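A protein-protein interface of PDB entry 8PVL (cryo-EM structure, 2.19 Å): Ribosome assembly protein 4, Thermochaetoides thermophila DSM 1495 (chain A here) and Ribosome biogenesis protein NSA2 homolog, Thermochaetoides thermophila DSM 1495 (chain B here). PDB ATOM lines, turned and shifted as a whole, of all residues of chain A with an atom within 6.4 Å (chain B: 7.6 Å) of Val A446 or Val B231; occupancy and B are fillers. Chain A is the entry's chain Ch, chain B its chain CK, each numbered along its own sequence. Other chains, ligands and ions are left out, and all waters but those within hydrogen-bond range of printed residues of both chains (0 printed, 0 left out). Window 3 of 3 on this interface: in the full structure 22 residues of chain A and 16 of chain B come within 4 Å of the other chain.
ND2 of Asn A426 is in hydrogen-bond range of O of Val A446 (3.2 Å). OD2 of Asp A467 lies within hydrogen-bond range of ND1 of His A445 (3.1 Å). OG1 of Thr A469 sits close to ND1 of His A445. N of Val A446 sits at hydrogen-bond distance from OD2 of Asp A467, 3.3 Å away. OG of Ser A465 sits close to N of Asp A467 (3.2 Å). The side-chain hydroxyl of Thr A469 lies within hydrogen-bond range of the side-chain carboxylate of Asp A467.
Val A446 touches just these residues of chain B: Gly B229 and Val B231. Printed residues of chain B within 4 Å of Asp A467: Val B231 (3.4 Å). Of the printed residues of chain B, Thr A469 touches Val B231 (3.7 Å). Printed residues of chain B within 4 Å of Pro A485: Ala B233 (3.7 Å) and Gly B235 (3.7 Å). Ser B226 touches none of the printed residues of chain A. Printed residues of chain A within 4 Å of Gly B229: Val A446. Of chain A, only Val A446 (3.9 Å), Asp A467 (3.4 Å) and Thr A469 (3.7 Å) come within 4 Å of Val B231. Of the printed residues of chain A, Gly B235 touches Pro A485. The nearest residue of chain B that does not touch Val A446 is Ile B237 (4.1 Å). The nearest residue of chain A that does not touch Val B231 is Pro A485 (5.4 Å). The nearest printed residue of chain B that does not touch Thr A469 is Gly B235 (5.7 Å).
Among the printed residues, merely in contact across the chains: Val A446 with Gly B229 (3.7 Å), Val A446 with Val B231 (3.9 Å), Asp A467 with Val B231 (3.4 Å), Thr A469 with Val B231 (3.7 Å), Pro A485 with Ala B233 (3.7 Å) and Pro A485 with Gly B235 (3.7 Å).
Along chain B the printed residues that touch a printed residue of chain A span positions 229 to 235. Printed residues of chain A that touch a printed residue of chain B: Val A446, Asp A467, Thr A469 and Pro A485. Hydrophobic or aromatic side chains of chain A that line the printed part of chain B: Val A446 and Pro A485. Along chain A the printed residues that touch a printed residue of chain B span positions 446 to 485. Among the printed residues, 6 pairs touch across the chains.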
ATOM      1  N   ASN A 426     -10.085 -19.774 -10.413  1.00  0.00           N
ATOM      2  CA  ASN A 426      -8.897 -20.525 -10.831  1.00  0.00           C
ATOM      3  C   ASN A 426      -7.630 -20.020 -10.148  1.00  0.00           C
ATOM      4  O   ASN A 426      -6.538 -20.107 -10.710  1.00  0.00           O
ATOM      5  CB  ASN A 426      -8.707 -20.514 -12.355  1.00  0.00           C
ATOM      6  CG  ASN A 426     -10.014 -20.582 -13.114  1.00  0.00           C
ATOM      7  OD1 ASN A 426     -11.026 -21.044 -12.597  1.00  0.00           O
ATOM      8  ND2 ASN A 426      -9.991 -20.131 -14.358  1.00  0.00           N
ATOM      9  N   GLY A 444      -1.787 -20.701 -11.884  1.00  0.00           N
ATOM     10  CA  GLY A 444      -1.491 -21.757 -12.831  1.00  0.00           C
ATOM     11  C   GLY A 444      -2.686 -22.593 -13.237  1.00  0.00           C
ATOM     12  O   GLY A 444      -2.646 -23.277 -14.263  1.00  0.00           O
ATOM     13  N   HIS A 445      -3.765 -22.532 -12.466  1.00  0.00           N
ATOM     14  CA  HIS A 445      -4.922 -23.369 -12.739  1.00  0.00           C
ATOM     15  C   HIS A 445      -5.854 -22.685 -13.731  1.00  0.00           C
ATOM     16  O   HIS A 445      -5.922 -21.457 -13.810  1.00  0.00           O
ATOM     17  CB  HIS A 445      -5.675 -23.696 -11.448  1.00  0.00           C
ATOM     18  CG  HIS A 445      -5.029 -24.765 -10.623  1.00  0.00           C
ATOM     19  ND1 HIS A 445      -4.887 -26.063 -11.065  1.00  0.00           N
ATOM     20  CD2 HIS A 445      -4.492 -24.732  -9.381  1.00  0.00           C
ATOM     21  CE1 HIS A 445      -4.288 -26.781 -10.132  1.00  0.00           C
ATOM     22  NE2 HIS A 445      -4.040 -25.997  -9.099  1.00  0.00           N
ATOM     23  N   VAL A 446      -6.571 -23.502 -14.501  1.00  0.00           N
ATOM     24  CA  VAL A 446      -7.494 -23.016 -15.519  1.00  0.00           C
ATOM     25  C   VAL A 446      -8.941 -23.309 -15.173  1.00  0.00           C
ATOM     26  O   VAL A 446      -9.842 -22.909 -15.921  1.00  0.00           O
ATOM     27  CB  VAL A 446      -7.147 -23.592 -16.905  1.00  0.00           C
ATOM     28  CG1 VAL A 446      -5.946 -22.876 -17.485  1.00  0.00           C
ATOM     29  CG2 VAL A 446      -6.881 -25.081 -16.810  1.00  0.00           C
ATOM     30  N   ALA A 447      -9.190 -23.992 -14.069  1.00  0.00           N
ATOM     31  CA  ALA A 447     -10.515 -24.336 -13.575  1.00  0.00           C
ATOM     32  C   ALA A 447     -10.548 -23.990 -12.099  1.00  0.00           C
ATOM     33  O   ALA A 447      -9.498 -23.733 -11.500  1.00  0.00           O
ATOM     34  CB  ALA A 447     -10.801 -25.828 -13.811  1.00  0.00           C
ATOM     35  N   PRO A 448     -11.741 -23.881 -11.498  1.00  0.00           N
ATOM     36  CA  PRO A 448     -11.826 -23.562 -10.065  1.00  0.00           C
ATOM     37  C   PRO A 448     -11.037 -24.516  -9.178  1.00  0.00           C
ATOM     38  O   PRO A 448     -11.115 -25.738  -9.315  1.00  0.00           O
ATOM     39  CB  PRO A 448     -13.326 -23.659  -9.781  1.00  0.00           C
ATOM     40  CG  PRO A 448     -13.957 -23.256 -11.041  1.00  0.00           C
ATOM     41  CD  PRO A 448     -13.048 -23.687 -12.159  1.00  0.00           C
ATOM     42  N   SER A 465      -7.422 -29.090  -8.205  1.00  0.00           N
ATOM     43  CA  SER A 465      -8.417 -28.277  -8.890  1.00  0.00           C
ATOM     44  C   SER A 465      -9.340 -29.117  -9.762  1.00  0.00           C
ATOM     45  O   SER A 465      -9.174 -30.328  -9.919  1.00  0.00           O
ATOM     46  CB  SER A 465      -7.751 -27.194  -9.741  1.00  0.00           C
ATOM     47  OG  SER A 465      -8.676 -26.631 -10.651  1.00  0.00           O
ATOM     48  N   ASP A 467      -9.501 -28.794 -12.918  1.00  0.00           N
ATOM     49  CA  ASP A 467      -8.822 -29.073 -14.180  1.00  0.00           C
ATOM     50  C   ASP A 467      -8.030 -30.377 -14.161  1.00  0.00           C
ATOM     51  O   ASP A 467      -7.114 -30.529 -14.978  1.00  0.00           O
ATOM     52  CB  ASP A 467      -7.908 -27.900 -14.576  1.00  0.00           C
ATOM     53  CG  ASP A 467      -6.777 -27.642 -13.582  1.00  0.00           C
ATOM     54  OD1 ASP A 467      -6.664 -28.329 -12.546  1.00  0.00           O
ATOM     55  OD2 ASP A 467      -5.977 -26.723 -13.851  1.00  0.00           O
ATOM     56  N   CYS A 468      -8.347 -31.278 -13.227  1.00  0.00           N
ATOM     57  CA  CYS A 468      -7.776 -32.615 -13.091  1.00  0.00           C
ATOM     58  C   CYS A 468      -6.293 -32.594 -12.750  1.00  0.00           C
ATOM     59  O   CYS A 468      -5.579 -33.555 -13.048  1.00  0.00           O
ATOM     60  CB  CYS A 468      -8.009 -33.461 -14.353  1.00  0.00           C
ATOM     61  SG  CYS A 468      -9.615 -33.227 -15.152  1.00  0.00           S
ATOM     62  N   THR A 469      -5.799 -31.523 -12.130  1.00  0.00           N
ATOM     63  CA  THR A 469      -4.386 -31.418 -11.798  1.00  0.00           C
ATOM     64  C   THR A 469      -4.183 -31.029 -10.338  1.00  0.00           C
ATOM     65  O   THR A 469      -5.048 -30.421  -9.682  1.00  0.00           O
ATOM     66  CB  THR A 469      -3.637 -30.396 -12.680  1.00  0.00           C
ATOM     67  OG1 THR A 469      -4.052 -29.066 -12.346  1.00  0.00           O
ATOM     68  CG2 THR A 469      -3.856 -30.653 -14.165  1.00  0.00           C
ATOM     69  N   LYS A 471      -1.054 -28.943  -8.147  1.00  0.00           N
ATOM     70  CA  LYS A 471       0.072 -28.039  -8.340  1.00  0.00           C
ATOM     71  C   LYS A 471       0.728 -27.750  -7.003  1.00  0.00           C
ATOM     72  O   LYS A 471       0.051 -27.356  -6.051  1.00  0.00           O
ATOM     73  CB  LYS A 471      -0.368 -26.735  -9.014  1.00  0.00           C
ATOM     74  CG  LYS A 471      -0.761 -26.910 -10.466  1.00  0.00           C
ATOM     75  CD  LYS A 471      -0.800 -25.604 -11.214  1.00  0.00           C
ATOM     76  CE  LYS A 471      -1.487 -25.794 -12.546  1.00  0.00           C
ATOM     77  NZ  LYS A 471      -1.024 -27.020 -13.239  1.00  0.00           N
ATOM     78  N   ASP A 483       4.281 -29.480 -11.162  1.00  0.00           N
ATOM     79  CA  ASP A 483       2.998 -29.757 -11.794  1.00  0.00           C
ATOM     80  C   ASP A 483       2.741 -31.255 -11.731  1.00  0.00           C
ATOM     81  O   ASP A 483       3.608 -32.049 -12.108  1.00  0.00           O
ATOM     82  CB  ASP A 483       2.989 -29.276 -13.245  1.00  0.00           C
ATOM     83  CG  ASP A 483       1.613 -28.861 -13.714  1.00  0.00           C
ATOM     84  OD1 ASP A 483       0.615 -29.328 -13.129  1.00  0.00           O
ATOM     85  OD2 ASP A 483       1.528 -28.069 -14.674  1.00  0.00           O
ATOM     86  N   PRO A 485       0.133 -33.792 -13.145  1.00  0.00           N
ATOM     87  CA  PRO A 485      -0.986 -34.324 -13.921  1.00  0.00           C
ATOM     88  C   PRO A 485      -1.102 -35.833 -13.749  1.00  0.00           C
ATOM     89  O   PRO A 485      -0.204 -36.504 -13.242  1.00  0.00           O
ATOM     90  CB  PRO A 485      -0.606 -33.974 -15.372  1.00  0.00           C
ATOM     91  CG  PRO A 485       0.731 -33.243 -15.289  1.00  0.00           C
ATOM     92  CD  PRO A 485       1.327 -33.624 -13.983  1.00  0.00           C
ATOM     93  N   VAL B 225     -10.648 -22.816 -26.581  1.00  0.00           N
ATOM     94  CA  VAL B 225     -11.288 -23.536 -25.487  1.00  0.00           C
ATOM     95  C   VAL B 225     -10.570 -23.238 -24.178  1.00  0.00           C
ATOM     96  O   VAL B 225     -10.517 -24.087 -23.281  1.00  0.00           O
ATOM     97  CB  VAL B 225     -11.331 -25.050 -25.766  1.00  0.00           C
ATOM     98  CG1 VAL B 225     -12.377 -25.362 -26.821  1.00  0.00           C
ATOM     99  CG2 VAL B 225      -9.969 -25.553 -26.207  1.00  0.00           C
ATOM    100  N   SER B 226     -10.005 -22.032 -24.064  1.00  0.00           N
ATOM    101  CA  SER B 226      -9.353 -21.620 -22.825  1.00  0.00           C
ATOM    102  C   SER B 226     -10.339 -21.524 -21.669  1.00  0.00           C
ATOM    103  O   SER B 226      -9.967 -21.769 -20.516  1.00  0.00           O
ATOM    104  CB  SER B 226      -8.649 -20.277 -23.021  1.00  0.00           C
ATOM    105  OG  SER B 226      -7.641 -20.368 -24.009  1.00  0.00           O
ATOM    106  N   ASP B 227     -11.593 -21.165 -21.953  1.00  0.00           N
ATOM    107  CA  ASP B 227     -12.595 -21.037 -20.901  1.00  0.00           C
ATOM    108  C   ASP B 227     -12.981 -22.388 -20.311  1.00  0.00           C
ATOM    109  O   ASP B 227     -13.375 -22.461 -19.143  1.00  0.00           O
ATOM    110  CB  ASP B 227     -13.837 -20.333 -21.446  1.00  0.00           C
ATOM    111  CG  ASP B 227     -13.787 -18.834 -21.252  1.00  0.00           C
ATOM    112  OD1 ASP B 227     -12.698 -18.246 -21.414  1.00  0.00           O
ATOM    113  OD2 ASP B 227     -14.841 -18.239 -20.945  1.00  0.00           O
ATOM    114  N   LEU B 228     -12.882 -23.459 -21.096  1.00  0.00           N
ATOM    115  CA  LEU B 228     -13.301 -24.773 -20.628  1.00  0.00           C
ATOM    116  C   LEU B 228     -12.294 -25.424 -19.692  1.00  0.00           C
ATOM    117  O   LEU B 228     -12.660 -26.356 -18.966  1.00  0.00           O
ATOM    118  CB  LEU B 228     -13.569 -25.686 -21.824  1.00  0.00           C
ATOM    119  CG  LEU B 228     -14.796 -25.285 -22.643  1.00  0.00           C
ATOM    120  CD1 LEU B 228     -14.773 -25.942 -24.003  1.00  0.00           C
ATOM    121  CD2 LEU B 228     -16.065 -25.648 -21.897  1.00  0.00           C
ATOM    122  N   GLY B 229     -11.046 -24.960 -19.686  1.00  0.00           N
ATOM    123  CA  GLY B 229     -10.038 -25.479 -18.782  1.00  0.00           C
ATOM    124  C   GLY B 229      -9.650 -26.919 -19.047  1.00  0.00           C
ATOM    125  O   GLY B 229      -9.850 -27.787 -18.192  1.00  0.00           O
ATOM    126  N   ILE B 230      -9.091 -27.186 -20.221  1.00  0.00           N
ATOM    127  CA  ILE B 230      -8.745 -28.539 -20.642  1.00  0.00           C
ATOM    128  C   ILE B 230      -7.235 -28.701 -20.541  1.00  0.00           C
ATOM    129  O   ILE B 230      -6.476 -27.955 -21.171  1.00  0.00           O
ATOM    130  CB  ILE B 230      -9.241 -28.826 -22.066  1.00  0.00           C
ATOM    131  CG1 ILE B 230     -10.746 -28.567 -22.161  1.00  0.00           C
ATOM    132  CG2 ILE B 230      -8.919 -30.252 -22.466  1.00  0.00           C
ATOM    133  CD1 ILE B 230     -11.287 -28.630 -23.566  1.00  0.00           C
ATOM    134  N   VAL B 231      -6.799 -29.680 -19.754  1.00  0.00           N
ATOM    135  CA  VAL B 231      -5.387 -29.972 -19.540  1.00  0.00           C
ATOM    136  C   VAL B 231      -5.088 -31.330 -20.155  1.00  0.00           C
ATOM    137  O   VAL B 231      -5.833 -32.293 -19.939  1.00  0.00           O
ATOM    138  CB  VAL B 231      -5.027 -29.954 -18.044  1.00  0.00           C
ATOM    139  CG1 VAL B 231      -3.531 -30.120 -17.851  1.00  0.00           C
ATOM    140  CG2 VAL B 231      -5.508 -28.669 -17.398  1.00  0.00           C
ATOM    141  N   THR B 232      -4.005 -31.409 -20.924  1.00  0.00           N
ATOM    142  CA  THR B 232      -3.614 -32.658 -21.555  1.00  0.00           C
ATOM    143  C   THR B 232      -2.945 -33.580 -20.535  1.00  0.00           C
ATOM    144  O   THR B 232      -2.752 -33.228 -19.369  1.00  0.00           O
ATOM    145  CB  THR B 232      -2.691 -32.394 -22.743  1.00  0.00           C
ATOM    146  OG1 THR B 232      -1.367 -32.114 -22.273  1.00  0.00           O
ATOM    147  CG2 THR B 232      -3.197 -31.219 -23.564  1.00  0.00           C
ATOM    148  N   ALA B 233      -2.587 -34.784 -20.988  1.00  0.00           N
ATOM    149  CA  ALA B 233      -1.984 -35.768 -20.095  1.00  0.00           C
ATOM    150  C   ALA B 233      -0.581 -35.361 -19.662  1.00  0.00           C
ATOM    151  O   ALA B 233      -0.129 -35.763 -18.584  1.00  0.00           O
ATOM    152  CB  ALA B 233      -1.954 -37.139 -20.770  1.00  0.00           C
ATOM    153  N   SER B 234       0.115 -34.570 -20.471  1.00  0.00           N
ATOM    154  CA  SER B 234       1.442 -34.080 -20.129  1.00  0.00           C
ATOM    155  C   SER B 234       1.402 -32.765 -19.360  1.00  0.00           C
ATOM    156  O   SER B 234       2.457 -32.176 -19.109  1.00  0.00           O
ATOM    157  CB  SER B 234       2.287 -33.922 -21.394  1.00  0.00           C
ATOM    158  OG  SER B 234       2.061 -32.665 -22.007  1.00  0.00           O
ATOM    159  N   GLY B 235       0.215 -32.295 -18.987  1.00  0.00           N
ATOM    160  CA  GLY B 235       0.073 -31.082 -18.215  1.00  0.00           C
ATOM    161  C   GLY B 235      -0.059 -29.810 -19.019  1.00  0.00           C
ATOM    162  O   GLY B 235      -0.256 -28.743 -18.425  1.00  0.00           O
ATOM    163  N   LYS B 236       0.042 -29.880 -20.340  1.00  0.00           N
ATOM    164  CA  LYS B 236      -0.088 -28.694 -21.169  1.00  0.00           C
ATOM    165  C   LYS B 236      -1.547 -28.264 -21.265  1.00  0.00           C
ATOM    166  O   LYS B 236      -2.467 -29.071 -21.115  1.00  0.00           O
ATOM    167  CB  LYS B 236       0.479 -28.948 -22.563  1.00  0.00           C
ATOM    168  CG  LYS B 236       1.921 -28.508 -22.723  1.00  0.00           C
ATOM    169  CD  LYS B 236       2.420 -28.753 -24.134  1.00  0.00           C
ATOM    170  CE  LYS B 236       3.917 -28.998 -24.147  1.00  0.00           C
ATOM    171  NZ  LYS B 236       4.276 -30.225 -23.389  1.00  0.00           N
ATOM    172  N   ILE B 237      -1.748 -26.977 -21.514  1.00  0.00           N
ATOM    173  CA  ILE B 237      -3.086 -26.407 -21.619  1.00  0.00           C
ATOM    174  C   ILE B 237      -3.520 -26.444 -23.077  1.00  0.00           C
ATOM    175  O   ILE B 237      -2.908 -25.797 -23.933  1.00  0.00           O
ATOM    176  CB  ILE B 237      -3.126 -24.972 -21.073  1.00  0.00           C
ATOM    177  CG1 ILE B 237      -2.615 -24.928 -19.633  1.00  0.00           C
ATOM    178  CG2 ILE B 237      -4.534 -24.414 -21.159  1.00  0.00           C
ATOM    179  CD1 ILE B 237      -3.355 -25.848 -18.695  1.00  0.00           C
ATOM    180  N   ALA B 238      -4.578 -27.195 -23.361  1.00  0.00           N
ATOM    181  CA  ALA B 238      -5.198 -27.157 -24.677  1.00  0.00           C
ATOM    182  C   ALA B 238      -6.066 -25.910 -24.773  1.00  0.00           C
ATOM    183  O   ALA B 238      -6.968 -25.711 -23.954  1.00  0.00           O
ATOM    184  CB  ALA B 238      -6.029 -28.414 -24.916  1.00  0.00           C
